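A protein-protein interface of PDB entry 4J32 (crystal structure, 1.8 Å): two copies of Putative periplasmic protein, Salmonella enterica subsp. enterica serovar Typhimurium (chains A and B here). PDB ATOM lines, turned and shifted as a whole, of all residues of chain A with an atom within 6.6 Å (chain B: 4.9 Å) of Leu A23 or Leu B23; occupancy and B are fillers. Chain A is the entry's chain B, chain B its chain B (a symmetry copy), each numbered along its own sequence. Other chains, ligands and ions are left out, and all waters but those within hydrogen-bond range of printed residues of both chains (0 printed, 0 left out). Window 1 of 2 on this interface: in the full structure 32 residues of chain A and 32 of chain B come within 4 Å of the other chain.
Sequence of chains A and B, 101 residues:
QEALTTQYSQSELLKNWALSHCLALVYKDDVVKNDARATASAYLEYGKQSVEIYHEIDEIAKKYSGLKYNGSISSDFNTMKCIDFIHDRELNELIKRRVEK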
ATOM      1  N   ALA A  18     -25.925  -7.062  10.057  1.00  0.00           N
ATOM      2  CA  ALA A  18     -26.024  -5.605  10.145  1.00  0.00           C
ATOM      3  C   ALA A  18     -25.147  -4.920   9.072  1.00  0.00           C
ATOM      4  O   ALA A  18     -25.606  -4.005   8.349  1.00  0.00           O
ATOM      5  CB  ALA A  18     -25.627  -5.145  11.568  1.00  0.00           C
ATOM      6  N   LEU A  19     -23.901  -5.359   8.965  1.00  0.00           N
ATOM      7  CA  LEU A  19     -22.976  -4.758   8.016  1.00  0.00           C
ATOM      8  C   LEU A  19     -23.429  -4.951   6.554  1.00  0.00           C
ATOM      9  O   LEU A  19     -23.508  -3.969   5.787  1.00  0.00           O
ATOM     10  CB  LEU A  19     -21.564  -5.309   8.231  1.00  0.00           C
ATOM     11  CG  LEU A  19     -20.497  -4.859   7.221  1.00  0.00           C
ATOM     12  CD1 LEU A  19     -20.410  -3.292   7.136  1.00  0.00           C
ATOM     13  CD2 LEU A  19     -19.155  -5.483   7.641  1.00  0.00           C
ATOM     14  N   SER A  20     -23.740  -6.195   6.180  1.00  0.00           N
ATOM     15  CA  SER A  20     -24.133  -6.471   4.796  1.00  0.00           C
ATOM     16  C   SER A  20     -25.443  -5.788   4.437  1.00  0.00           C
ATOM     17  O   SER A  20     -25.563  -5.257   3.326  1.00  0.00           O
ATOM     18  CB  SER A  20     -24.174  -7.971   4.473  1.00  0.00           C
ATOM     19  OG  SER A  20     -24.814  -8.694   5.499  1.00  0.00           O
ATOM     20  N   HIS A  21     -26.401  -5.767   5.370  1.00  0.00           N
ATOM     21  CA  HIS A  21     -27.663  -5.076   5.124  1.00  0.00           C
ATOM     22  C   HIS A  21     -27.431  -3.578   4.886  1.00  0.00           C
ATOM     23  O   HIS A  21     -28.012  -2.992   3.968  1.00  0.00           O
ATOM     24  CB  HIS A  21     -28.650  -5.287   6.274  1.00  0.00           C
ATOM     25  CG  HIS A  21     -29.949  -4.580   6.071  1.00  0.00           C
ATOM     26  ND1 HIS A  21     -30.870  -4.978   5.127  1.00  0.00           N
ATOM     27  CD2 HIS A  21     -30.469  -3.486   6.672  1.00  0.00           C
ATOM     28  CE1 HIS A  21     -31.911  -4.163   5.166  1.00  0.00           C
ATOM     29  NE2 HIS A  21     -31.680  -3.236   6.081  1.00  0.00           N
ATOM     30  N   CYS A  22     -26.592  -2.971   5.722  1.00  0.00           N
ATOM     31  CA  CYS A  22     -26.325  -1.538   5.569  1.00  0.00           C
ATOM     32  C   CYS A  22     -25.693  -1.249   4.198  1.00  0.00           C
ATOM     33  O   CYS A  22     -26.055  -0.270   3.520  1.00  0.00           O
ATOM     34  CB  CYS A  22     -25.417  -1.064   6.691  1.00  0.00           C
ATOM     35  SG  CYS A  22     -25.044   0.700   6.611  1.00  0.00           S
ATOM     36  N   LEU A  23     -24.777  -2.117   3.781  1.00  0.00           N
ATOM     37  CA  LEU A  23     -24.137  -1.949   2.460  1.00  0.00           C
ATOM     38  C   LEU A  23     -25.186  -2.066   1.338  1.00  0.00           C
ATOM     39  O   LEU A  23     -25.157  -1.298   0.361  1.00  0.00           O
ATOM     40  CB  LEU A  23     -22.992  -2.958   2.302  1.00  0.00           C
ATOM     41  CG  LEU A  23     -21.793  -2.790   3.242  1.00  0.00           C
ATOM     42  CD1 LEU A  23     -20.818  -4.007   3.129  1.00  0.00           C
ATOM     43  CD2 LEU A  23     -21.053  -1.438   2.955  1.00  0.00           C
ATOM     44  N   ALA A  24     -26.144  -2.984   1.505  1.00  0.00           N
ATOM     45  CA  ALA A  24     -27.270  -3.109   0.578  1.00  0.00           C
ATOM     46  C   ALA A  24     -28.126  -1.848   0.524  1.00  0.00           C
ATOM     47  O   ALA A  24     -28.748  -1.563  -0.496  1.00  0.00           O
ATOM     48  CB  ALA A  24     -28.154  -4.302   0.957  1.00  0.00           C
ATOM     49  N   LEU A  25     -28.207  -1.123   1.643  1.00  0.00           N
ATOM     50  CA  LEU A  25     -28.937   0.142   1.650  1.00  0.00           C
ATOM     51  C   LEU A  25     -28.219   1.303   0.961  1.00  0.00           C
ATOM     52  O   LEU A  25     -28.860   2.097   0.263  1.00  0.00           O
ATOM     53  CB  LEU A  25     -29.271   0.582   3.085  1.00  0.00           C
ATOM     54  CG  LEU A  25     -30.175  -0.322   3.928  1.00  0.00           C
ATOM     55  CD1 LEU A  25     -30.356   0.286   5.333  1.00  0.00           C
ATOM     56  CD2 LEU A  25     -31.513  -0.539   3.244  1.00  0.00           C
ATOM     57  N   VAL A  26     -26.925   1.448   1.201  1.00  0.00           N
ATOM     58  CA  VAL A  26     -26.223   2.677   0.812  1.00  0.00           C
ATOM     59  C   VAL A  26     -25.760   2.736  -0.647  1.00  0.00           C
ATOM     60  O   VAL A  26     -25.622   3.817  -1.203  1.00  0.00           O
ATOM     61  CB  VAL A  26     -25.040   3.047   1.762  1.00  0.00           C
ATOM     62  CG1 VAL A  26     -25.540   3.218   3.240  1.00  0.00           C
ATOM     63  CG2 VAL A  26     -23.914   2.023   1.685  1.00  0.00           C
ATOM     64  N   TYR A  27     -25.522   1.583  -1.251  1.00  0.00           N
ATOM     65  CA  TYR A  27     -24.959   1.539  -2.601  1.00  0.00           C
ATOM     66  C   TYR A  27     -26.076   1.555  -3.642  1.00  0.00           C
ATOM     67  O   TYR A  27     -27.125   0.958  -3.411  1.00  0.00           O
ATOM     68  CB  TYR A  27     -24.142   0.260  -2.756  1.00  0.00           C
ATOM     69  CG  TYR A  27     -22.844   0.202  -1.960  1.00  0.00           C
ATOM     70  CD1 TYR A  27     -21.999   1.325  -1.830  1.00  0.00           C
ATOM     71  CD2 TYR A  27     -22.450  -0.995  -1.380  1.00  0.00           C
ATOM     72  CE1 TYR A  27     -20.787   1.229  -1.120  1.00  0.00           C
ATOM     73  CE2 TYR A  27     -21.247  -1.112  -0.690  1.00  0.00           C
ATOM     74  CZ  TYR A  27     -20.426   0.001  -0.546  1.00  0.00           C
ATOM     75  OH  TYR A  27     -19.248  -0.192   0.145  1.00  0.00           O
ATOM     76  N   LYS A  28     -25.844   2.218  -4.767  1.00  0.00           N
ATOM     77  CA  LYS A  28     -26.879   2.390  -5.793  1.00  0.00           C
ATOM     78  C   LYS A  28     -26.924   1.213  -6.785  1.00  0.00           C
ATOM     79  O   LYS A  28     -28.010   0.731  -7.175  1.00  0.00           O
ATOM     80  CB  LYS A  28     -26.701   3.734  -6.517  1.00  0.00           C
ATOM     81  CG  LYS A  28     -27.927   4.114  -7.354  1.00  0.00           C
ATOM     82  CD  LYS A  28     -27.744   5.321  -8.262  1.00  0.00           C
ATOM     83  CE  LYS A  28     -29.058   5.576  -9.026  1.00  0.00           C
ATOM     84  NZ  LYS A  28     -28.941   6.520 -10.175  1.00  0.00           N
ATOM     85  N   VAL A  32     -24.180  -4.728  -7.017  1.00  0.00           N
ATOM     86  CA  VAL A  32     -23.678  -4.583  -5.627  1.00  0.00           C
ATOM     87  C   VAL A  32     -24.793  -4.729  -4.573  1.00  0.00           C
ATOM     88  O   VAL A  32     -24.626  -5.466  -3.579  1.00  0.00           O
ATOM     89  CB  VAL A  32     -22.903  -3.254  -5.448  1.00  0.00           C
ATOM     90  CG1 VAL A  32     -22.558  -3.010  -3.957  1.00  0.00           C
ATOM     91  CG2 VAL A  32     -21.650  -3.241  -6.355  1.00  0.00           C
ATOM     92  N   LYS A  33     -25.913  -4.019  -4.761  1.00  0.00           N
ATOM     93  CA  LYS A  33     -27.030  -4.109  -3.785  1.00  0.00           C
ATOM     94  C   LYS A  33     -27.504  -5.556  -3.667  1.00  0.00           C
ATOM     95  O   LYS A  33     -27.705  -6.040  -2.563  1.00  0.00           O
ATOM     96  CB  LYS A  33     -28.246  -3.258  -4.218  1.00  0.00           C
ATOM     97  CG  LYS A  33     -28.044  -1.766  -4.075  1.00  0.00           C
ATOM     98  CD  LYS A  33     -29.272  -0.947  -4.594  1.00  0.00           C
ATOM     99  CE  LYS A  33     -30.263  -0.649  -3.487  1.00  0.00           C
ATOM    100  NZ  LYS A  33     -29.627   0.091  -2.355  1.00  0.00           N
ATOM    101  N   ALA A  36     -24.929  -7.694  -1.674  1.00  0.00           N
ATOM    102  CA  ALA A  36     -25.022  -7.417  -0.251  1.00  0.00           C
ATOM    103  C   ALA A  36     -26.303  -8.021   0.358  1.00  0.00           C
ATOM    104  O   ALA A  36     -26.249  -8.572   1.453  1.00  0.00           O
ATOM    105  CB  ALA A  36     -24.908  -5.902   0.026  1.00  0.00           C
ATOM    106  N   ARG A  37     -27.426  -7.948  -0.355  1.00  0.00           N
ATOM    107  CA  ARG A  37     -28.685  -8.581   0.096  1.00  0.00           C
ATOM    108  C   ARG A  37     -28.539 -10.098   0.188  1.00  0.00           C
ATOM    109  O   ARG A  37     -29.009 -10.717   1.130  1.00  0.00           O
ATOM    110  CB  ARG A  37     -29.821  -8.285  -0.866  1.00  0.00           C
ATOM    111  CG  ARG A  37     -30.379  -6.923  -0.744  1.00  0.00           C
ATOM    112  CD  ARG A  37     -31.529  -6.813  -1.750  1.00  0.00           C
ATOM    113  NE  ARG A  37     -32.280  -5.589  -1.521  1.00  0.00           N
ATOM    114  CZ  ARG A  37     -33.513  -5.370  -1.975  1.00  0.00           C
ATOM    115  NH1 ARG A  37     -34.141  -6.288  -2.703  1.00  0.00           N
ATOM    116  NH2 ARG A  37     -34.126  -4.219  -1.700  1.00  0.00           N
ATOM    117  N   ASN A  78     -20.403   6.544   1.269  1.00  0.00           N
ATOM    118  CA  ASN A  78     -21.465   5.608   1.617  1.00  0.00           C
ATOM    119  C   ASN A  78     -20.912   4.447   2.447  1.00  0.00           C
ATOM    120  O   ASN A  78     -21.517   4.056   3.438  1.00  0.00           O
ATOM    121  CB  ASN A  78     -22.158   5.097   0.346  1.00  0.00           C
ATOM    122  CG  ASN A  78     -23.012   6.162  -0.292  1.00  0.00           C
ATOM    123  OD1 ASN A  78     -23.713   6.885   0.414  1.00  0.00           O
ATOM    124  ND2 ASN A  78     -22.956   6.279  -1.614  1.00  0.00           N
ATOM    125  N   THR A  79     -19.745   3.947   2.048  1.00  0.00           N
ATOM    126  CA  THR A  79     -19.124   2.794   2.726  1.00  0.00           C
ATOM    127  C   THR A  79     -18.902   3.183   4.194  1.00  0.00           C
ATOM    128  O   THR A  79     -19.114   2.387   5.102  1.00  0.00           O
ATOM    129  CB  THR A  79     -17.765   2.440   2.088  1.00  0.00           C
ATOM    130  OG1 THR A  79     -17.914   2.217   0.677  1.00  0.00           O
ATOM    131  CG2 THR A  79     -17.146   1.146   2.727  1.00  0.00           C
ATOM    132  N   MET A  80     -18.464   4.425   4.406  1.00  0.00           N
ATOM    133  CA  MET A  80     -18.174   4.939   5.749  1.00  0.00           C
ATOM    134  C   MET A  80     -19.392   4.968   6.675  1.00  0.00           C
ATOM    135  O   MET A  80     -19.267   4.797   7.914  1.00  0.00           O
ATOM    136  CB  MET A  80     -17.599   6.351   5.638  1.00  0.00           C
ATOM    137  CG  MET A  80     -17.036   6.847   6.933  1.00  0.00           C
ATOM    138  SD  MET A  80     -16.250   8.473   6.754  1.00  0.00           S
ATOM    139  CE  MET A  80     -14.664   7.982   6.062  1.00  0.00           C
ATOM    140  N   CYS A  82     -21.711   2.823   6.809  1.00  0.00           N
ATOM    141  CA  CYS A  82     -21.922   1.461   7.319  1.00  0.00           C
ATOM    142  C   CYS A  82     -20.827   1.043   8.293  1.00  0.00           C
ATOM    143  O   CYS A  82     -21.082   0.296   9.248  1.00  0.00           O
ATOM    144  CB  CYS A  82     -22.040   0.479   6.165  1.00  0.00           C
ATOM    145  SG  CYS A  82     -23.492   0.806   5.197  1.00  0.00           S
ATOM    146  N   ILE A  83     -19.614   1.552   8.083  1.00  0.00           N
ATOM    147  CA  ILE A  83     -18.532   1.260   9.035  1.00  0.00           C
ATOM    148  C   ILE A  83     -18.831   1.968  10.377  1.00  0.00           C
ATOM    149  O   ILE A  83     -18.682   1.375  11.448  1.00  0.00           O
ATOM    150  CB  ILE A  83     -17.129   1.614   8.451  1.00  0.00           C
ATOM    151  CG1 ILE A  83     -16.777   0.591   7.340  1.00  0.00           C
ATOM    152  CG2 ILE A  83     -16.048   1.584   9.567  1.00  0.00           C
ATOM    153  CD1 ILE A  83     -15.594   0.913   6.507  1.00  0.00           C
ATOM    154  N   LEU B  19     -11.466  -3.439   5.916  1.00  0.00           N
ATOM    155  CA  LEU B  19     -12.802  -3.700   5.403  1.00  0.00           C
ATOM    156  C   LEU B  19     -13.116  -2.874   4.137  1.00  0.00           C
ATOM    157  O   LEU B  19     -13.540  -3.439   3.109  1.00  0.00           O
ATOM    158  CB  LEU B  19     -13.847  -3.451   6.494  1.00  0.00           C
ATOM    159  CG  LEU B  19     -15.318  -3.568   6.065  1.00  0.00           C
ATOM    160  CD1 LEU B  19     -15.616  -4.961   5.402  1.00  0.00           C
ATOM    161  CD2 LEU B  19     -16.193  -3.329   7.308  1.00  0.00           C
ATOM    162  N   SER B  20     -12.890  -1.559   4.207  1.00  0.00           N
ATOM    163  CA  SER B  20     -13.206  -0.699   3.065  1.00  0.00           C
ATOM    164  C   SER B  20     -12.336  -1.018   1.860  1.00  0.00           C
ATOM    165  O   SER B  20     -12.845  -1.030   0.733  1.00  0.00           O
ATOM    166  CB  SER B  20     -13.158   0.797   3.411  1.00  0.00           C
ATOM    167  OG  SER B  20     -12.016   1.105   4.175  1.00  0.00           O
ATOM    168  N   HIS B  21     -11.051  -1.308   2.090  1.00  0.00           N
ATOM    169  CA  HIS B  21     -10.166  -1.689   0.993  1.00  0.00           C
ATOM    170  C   HIS B  21     -10.656  -2.974   0.313  1.00  0.00           C
ATOM    171  O   HIS B  21     -10.679  -3.061  -0.918  1.00  0.00           O
ATOM    172  CB  HIS B  21      -8.722  -1.855   1.471  1.00  0.00           C
ATOM    173  CG  HIS B  21      -7.786  -2.263   0.381  1.00  0.00           C
ATOM    174  ND1 HIS B  21      -7.416  -1.410  -0.636  1.00  0.00           N
ATOM    175  CD2 HIS B  21      -7.167  -3.439   0.136  1.00  0.00           C
ATOM    176  CE1 HIS B  21      -6.595  -2.043  -1.456  1.00  0.00           C
ATOM    177  NE2 HIS B  21      -6.446  -3.284  -1.020  1.00  0.00           N
ATOM    178  N   CYS B  22     -11.033  -3.962   1.120  1.00  0.00           N
ATOM    179  CA  CYS B  22     -11.504  -5.227   0.549  1.00  0.00           C
ATOM    180  C   CYS B  22     -12.761  -4.999  -0.305  1.00  0.00           C
ATOM    181  O   CYS B  22     -12.899  -5.566  -1.405  1.00  0.00           O
ATOM    182  CB  CYS B  22     -11.784  -6.219   1.664  1.00  0.00           C
ATOM    183  SG  CYS B  22     -12.347  -7.826   1.066  1.00  0.00           S
ATOM    184  N   LEU B  23     -13.656  -4.149   0.186  1.00  0.00           N
ATOM    185  CA  LEU B  23     -14.882  -3.834  -0.578  1.00  0.00           C
ATOM    186  C   LEU B  23     -14.523  -3.148  -1.909  1.00  0.00           C
ATOM    187  O   LEU B  23     -15.120  -3.446  -2.957  1.00  0.00           O
ATOM    188  CB  LEU B  23     -15.829  -2.987   0.283  1.00  0.00           C
ATOM    189  CG  LEU B  23     -16.415  -3.662   1.529  1.00  0.00           C
ATOM    190  CD1 LEU B  23     -17.170  -2.626   2.424  1.00  0.00           C
ATOM    191  CD2 LEU B  23     -17.349  -4.854   1.123  1.00  0.00           C
ATOM    192  N   ALA B  24     -13.509  -2.275  -1.881  1.00  0.00           N
ATOM    193  CA  ALA B  24     -12.986  -1.653  -3.098  1.00  0.00           C
ATOM    194  C   ALA B  24     -12.421  -2.674  -4.080  1.00  0.00           C
ATOM    195  O   ALA B  24     -12.425  -2.442  -5.286  1.00  0.00           O
ATOM    196  CB  ALA B  24     -11.900  -0.626  -2.758  1.00  0.00           C
ATOM    197  N   LEU B  25     -11.879  -3.779  -3.560  1.00  0.00           N
ATOM    198  CA  LEU B  25     -11.394  -4.842  -4.435  1.00  0.00           C
ATOM    199  C   LEU B  25     -12.487  -5.693  -5.082  1.00  0.00           C
ATOM    200  O   LEU B  25     -12.373  -6.053  -6.259  1.00  0.00           O
ATOM    201  CB  LEU B  25     -10.445  -5.790  -3.682  1.00  0.00           C
ATOM    202  CG  LEU B  25      -9.144  -5.213  -3.115  1.00  0.00           C
ATOM    203  CD1 LEU B  25      -8.362  -6.317  -2.378  1.00  0.00           C
ATOM    204  CD2 LEU B  25      -8.307  -4.582  -4.214  1.00  0.00           C
ATOM    205  N   VAL B  26     -13.498  -6.072  -4.315  1.00  0.00           N
ATOM    206  CA  VAL B  26     -14.436  -7.106  -4.768  1.00  0.00           C
ATOM    207  C   VAL B  26     -15.566  -6.615  -5.680  1.00  0.00           C
ATOM    208  O   VAL B  26     -16.084  -7.382  -6.479  1.00  0.00           O
ATOM    209  CB  VAL B  26     -15.026  -7.965  -3.606  1.00  0.00           C
ATOM    210  CG1 VAL B  26     -13.882  -8.667  -2.792  1.00  0.00           C
ATOM    211  CG2 VAL B  26     -15.915  -7.137  -2.686  1.00  0.00           C
ATOM    212  N   TYR B  27     -15.937  -5.351  -5.552  1.00  0.00           N
ATOM    213  CA  TYR B  27     -17.087  -4.824  -6.289  1.00  0.00           C
ATOM    214  C   TYR B  27     -16.644  -4.284  -7.646  1.00  0.00           C
ATOM    215  O   TYR B  27     -15.557  -3.717  -7.745  1.00  0.00           O
ATOM    216  CB  TYR B  27     -17.720  -3.697  -5.478  1.00  0.00           C
ATOM    217  CG  TYR B  27     -18.435  -4.119  -4.201  1.00  0.00           C
ATOM    218  CD1 TYR B  27     -19.227  -5.286  -4.141  1.00  0.00           C
ATOM    219  CD2 TYR B  27     -18.349  -3.319  -3.071  1.00  0.00           C
ATOM    220  CE1 TYR B  27     -19.907  -5.630  -2.958  1.00  0.00           C
ATOM    221  CE2 TYR B  27     -19.028  -3.634  -1.898  1.00  0.00           C
ATOM    222  CZ  TYR B  27     -19.791  -4.794  -1.836  1.00  0.00           C
ATOM    223  OH  TYR B  27     -20.440  -5.039  -0.644  1.00  0.00           O
ATOM    224  N   ALA B  36     -15.590   3.149  -1.784  1.00  0.00           N
ATOM    225  CA  ALA B  36     -14.836   2.327  -0.853  1.00  0.00           C
ATOM    226  C   ALA B  36     -13.362   2.772  -0.775  1.00  0.00           C
ATOM    227  O   ALA B  36     -12.802   2.816   0.316  1.00  0.00           O
ATOM    228  CB  ALA B  36     -14.971   0.829  -1.205  1.00  0.00           C
ATOM    229  N   THR B  79     -19.545  -9.506  -1.128  1.00  0.00           N
ATOM    230  CA  THR B  79     -19.610  -8.811   0.171  1.00  0.00           C
ATOM    231  C   THR B  79     -19.118  -9.791   1.247  1.00  0.00           C
ATOM    232  O   THR B  79     -18.393  -9.417   2.163  1.00  0.00           O
ATOM    233  CB  THR B  79     -21.055  -8.387   0.502  1.00  0.00           C
ATOM    234  OG1 THR B  79     -21.601  -7.590  -0.561  1.00  0.00           O
ATOM    235  CG2 THR B  79     -21.122  -7.548   1.828  1.00  0.00           C
ATOM    236  N   CYS B  82     -15.361 -10.213   2.002  1.00  0.00           N
ATOM    237  CA  CYS B  82     -14.770  -9.164   2.845  1.00  0.00           C
ATOM    238  C   CYS B  82     -15.181  -9.311   4.306  1.00  0.00           C
ATOM    239  O   CYS B  82     -14.402  -8.996   5.216  1.00  0.00           O
ATOM    240  CB  CYS B  82     -15.128  -7.789   2.305  1.00  0.00           C
ATOM    241  SG  CYS B  82     -14.396  -7.522   0.711  1.00  0.00           S
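The backbone NH (N) of Leu A23 is in hydrogen-bond range of the side-chain sulfur (SG) of Cys A82, 3.5 Å away. N of Leu B23 lies within hydrogen-bond range of SG of Cys B82 (3.5 Å). SG of Cys B22 forms a disulfide with SG of Cys B82. O of Tyr A27 sits at hydrogen-bond distance from NZ of Lys A33 (2.9 Å). The side-chain hydroxyl of Thr B79 sits at hydrogen-bond distance from the side-chain hydroxyl of Tyr B27. OH of Tyr A27 is in hydrogen-bond range of OG1 of Thr A79 (2.8 Å).
Leu A19 touches Leu B19 (CD2 to CD2, 3.7 Å). CD1 of Leu B23 touches CD1 of Leu A23, 3.96 Å away. CD1 of Leu A23 touches OH of Tyr B27, at 3.9 Å. CG2 of Thr B79 touches CD1 of Leu A23, 3.8 Å away. OH of Tyr A27 touches CD1 of Leu B23 (3.9 Å). Tyr A27 touches Tyr B27 (CE2 to CE2, 3.6 Å). CE1 of Tyr B27 touches CG1 of Val A32, at 3.9 Å. Thr B79 touches Ala A36 (OG1 to CA, 3.4 Å). Leu B23 touches Thr A79 (CD1 to CG2, 3.8 Å). CA of Ala B36 touches OG1 of Thr A79, at 3.4 Å.
Of the printed residues of chain B, Ala A36 touches Thr B79. Of the printed residues of chain A, Ser B20 touches Ile A83. Of the printed residues of chain A, Ala B36 touches Thr A79. Printed residues of chain A within 4 Å of Thr B79: Leu A23 and Ala A36. The nearest residue of chain A that does not touch Leu B23 is Ile A83 (5.6 Å).
Of the 12 printed residues of chain B, 6 touch a printed residue of chain A. Printed residues of chain B that touch a printed residue of chain A: Leu B19, Ser B20, Leu B23, Tyr B27, Ala B36 and Thr B79. Hydrophobic or aromatic side chains of chain B within 4 Å of the printed part of chain A: Leu B19, Leu B23, Tyr B27 and Ala B36. Along chain B the printed residues that touch a printed residue of chain A span positions 19 to 79. Of the 20 printed residues of chain A, 7 touch a printed residue of chain B. Among the printed residues, 12 pairs touch across the chains.
Leu B19 touches its own counterpart, Leu A19. Leu A23 touches Tyr B27, and with the chains exchanged Tyr A27 touches Leu B23. Leu A23 touches Thr B79, and with the chains exchanged Thr A79 touches Leu B23. Tyr B27 touches its own counterpart, Tyr A27. Of the 12 pairs that touch across the chains among the printed residues, 9 have their exchanged pair printed and touching as well.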
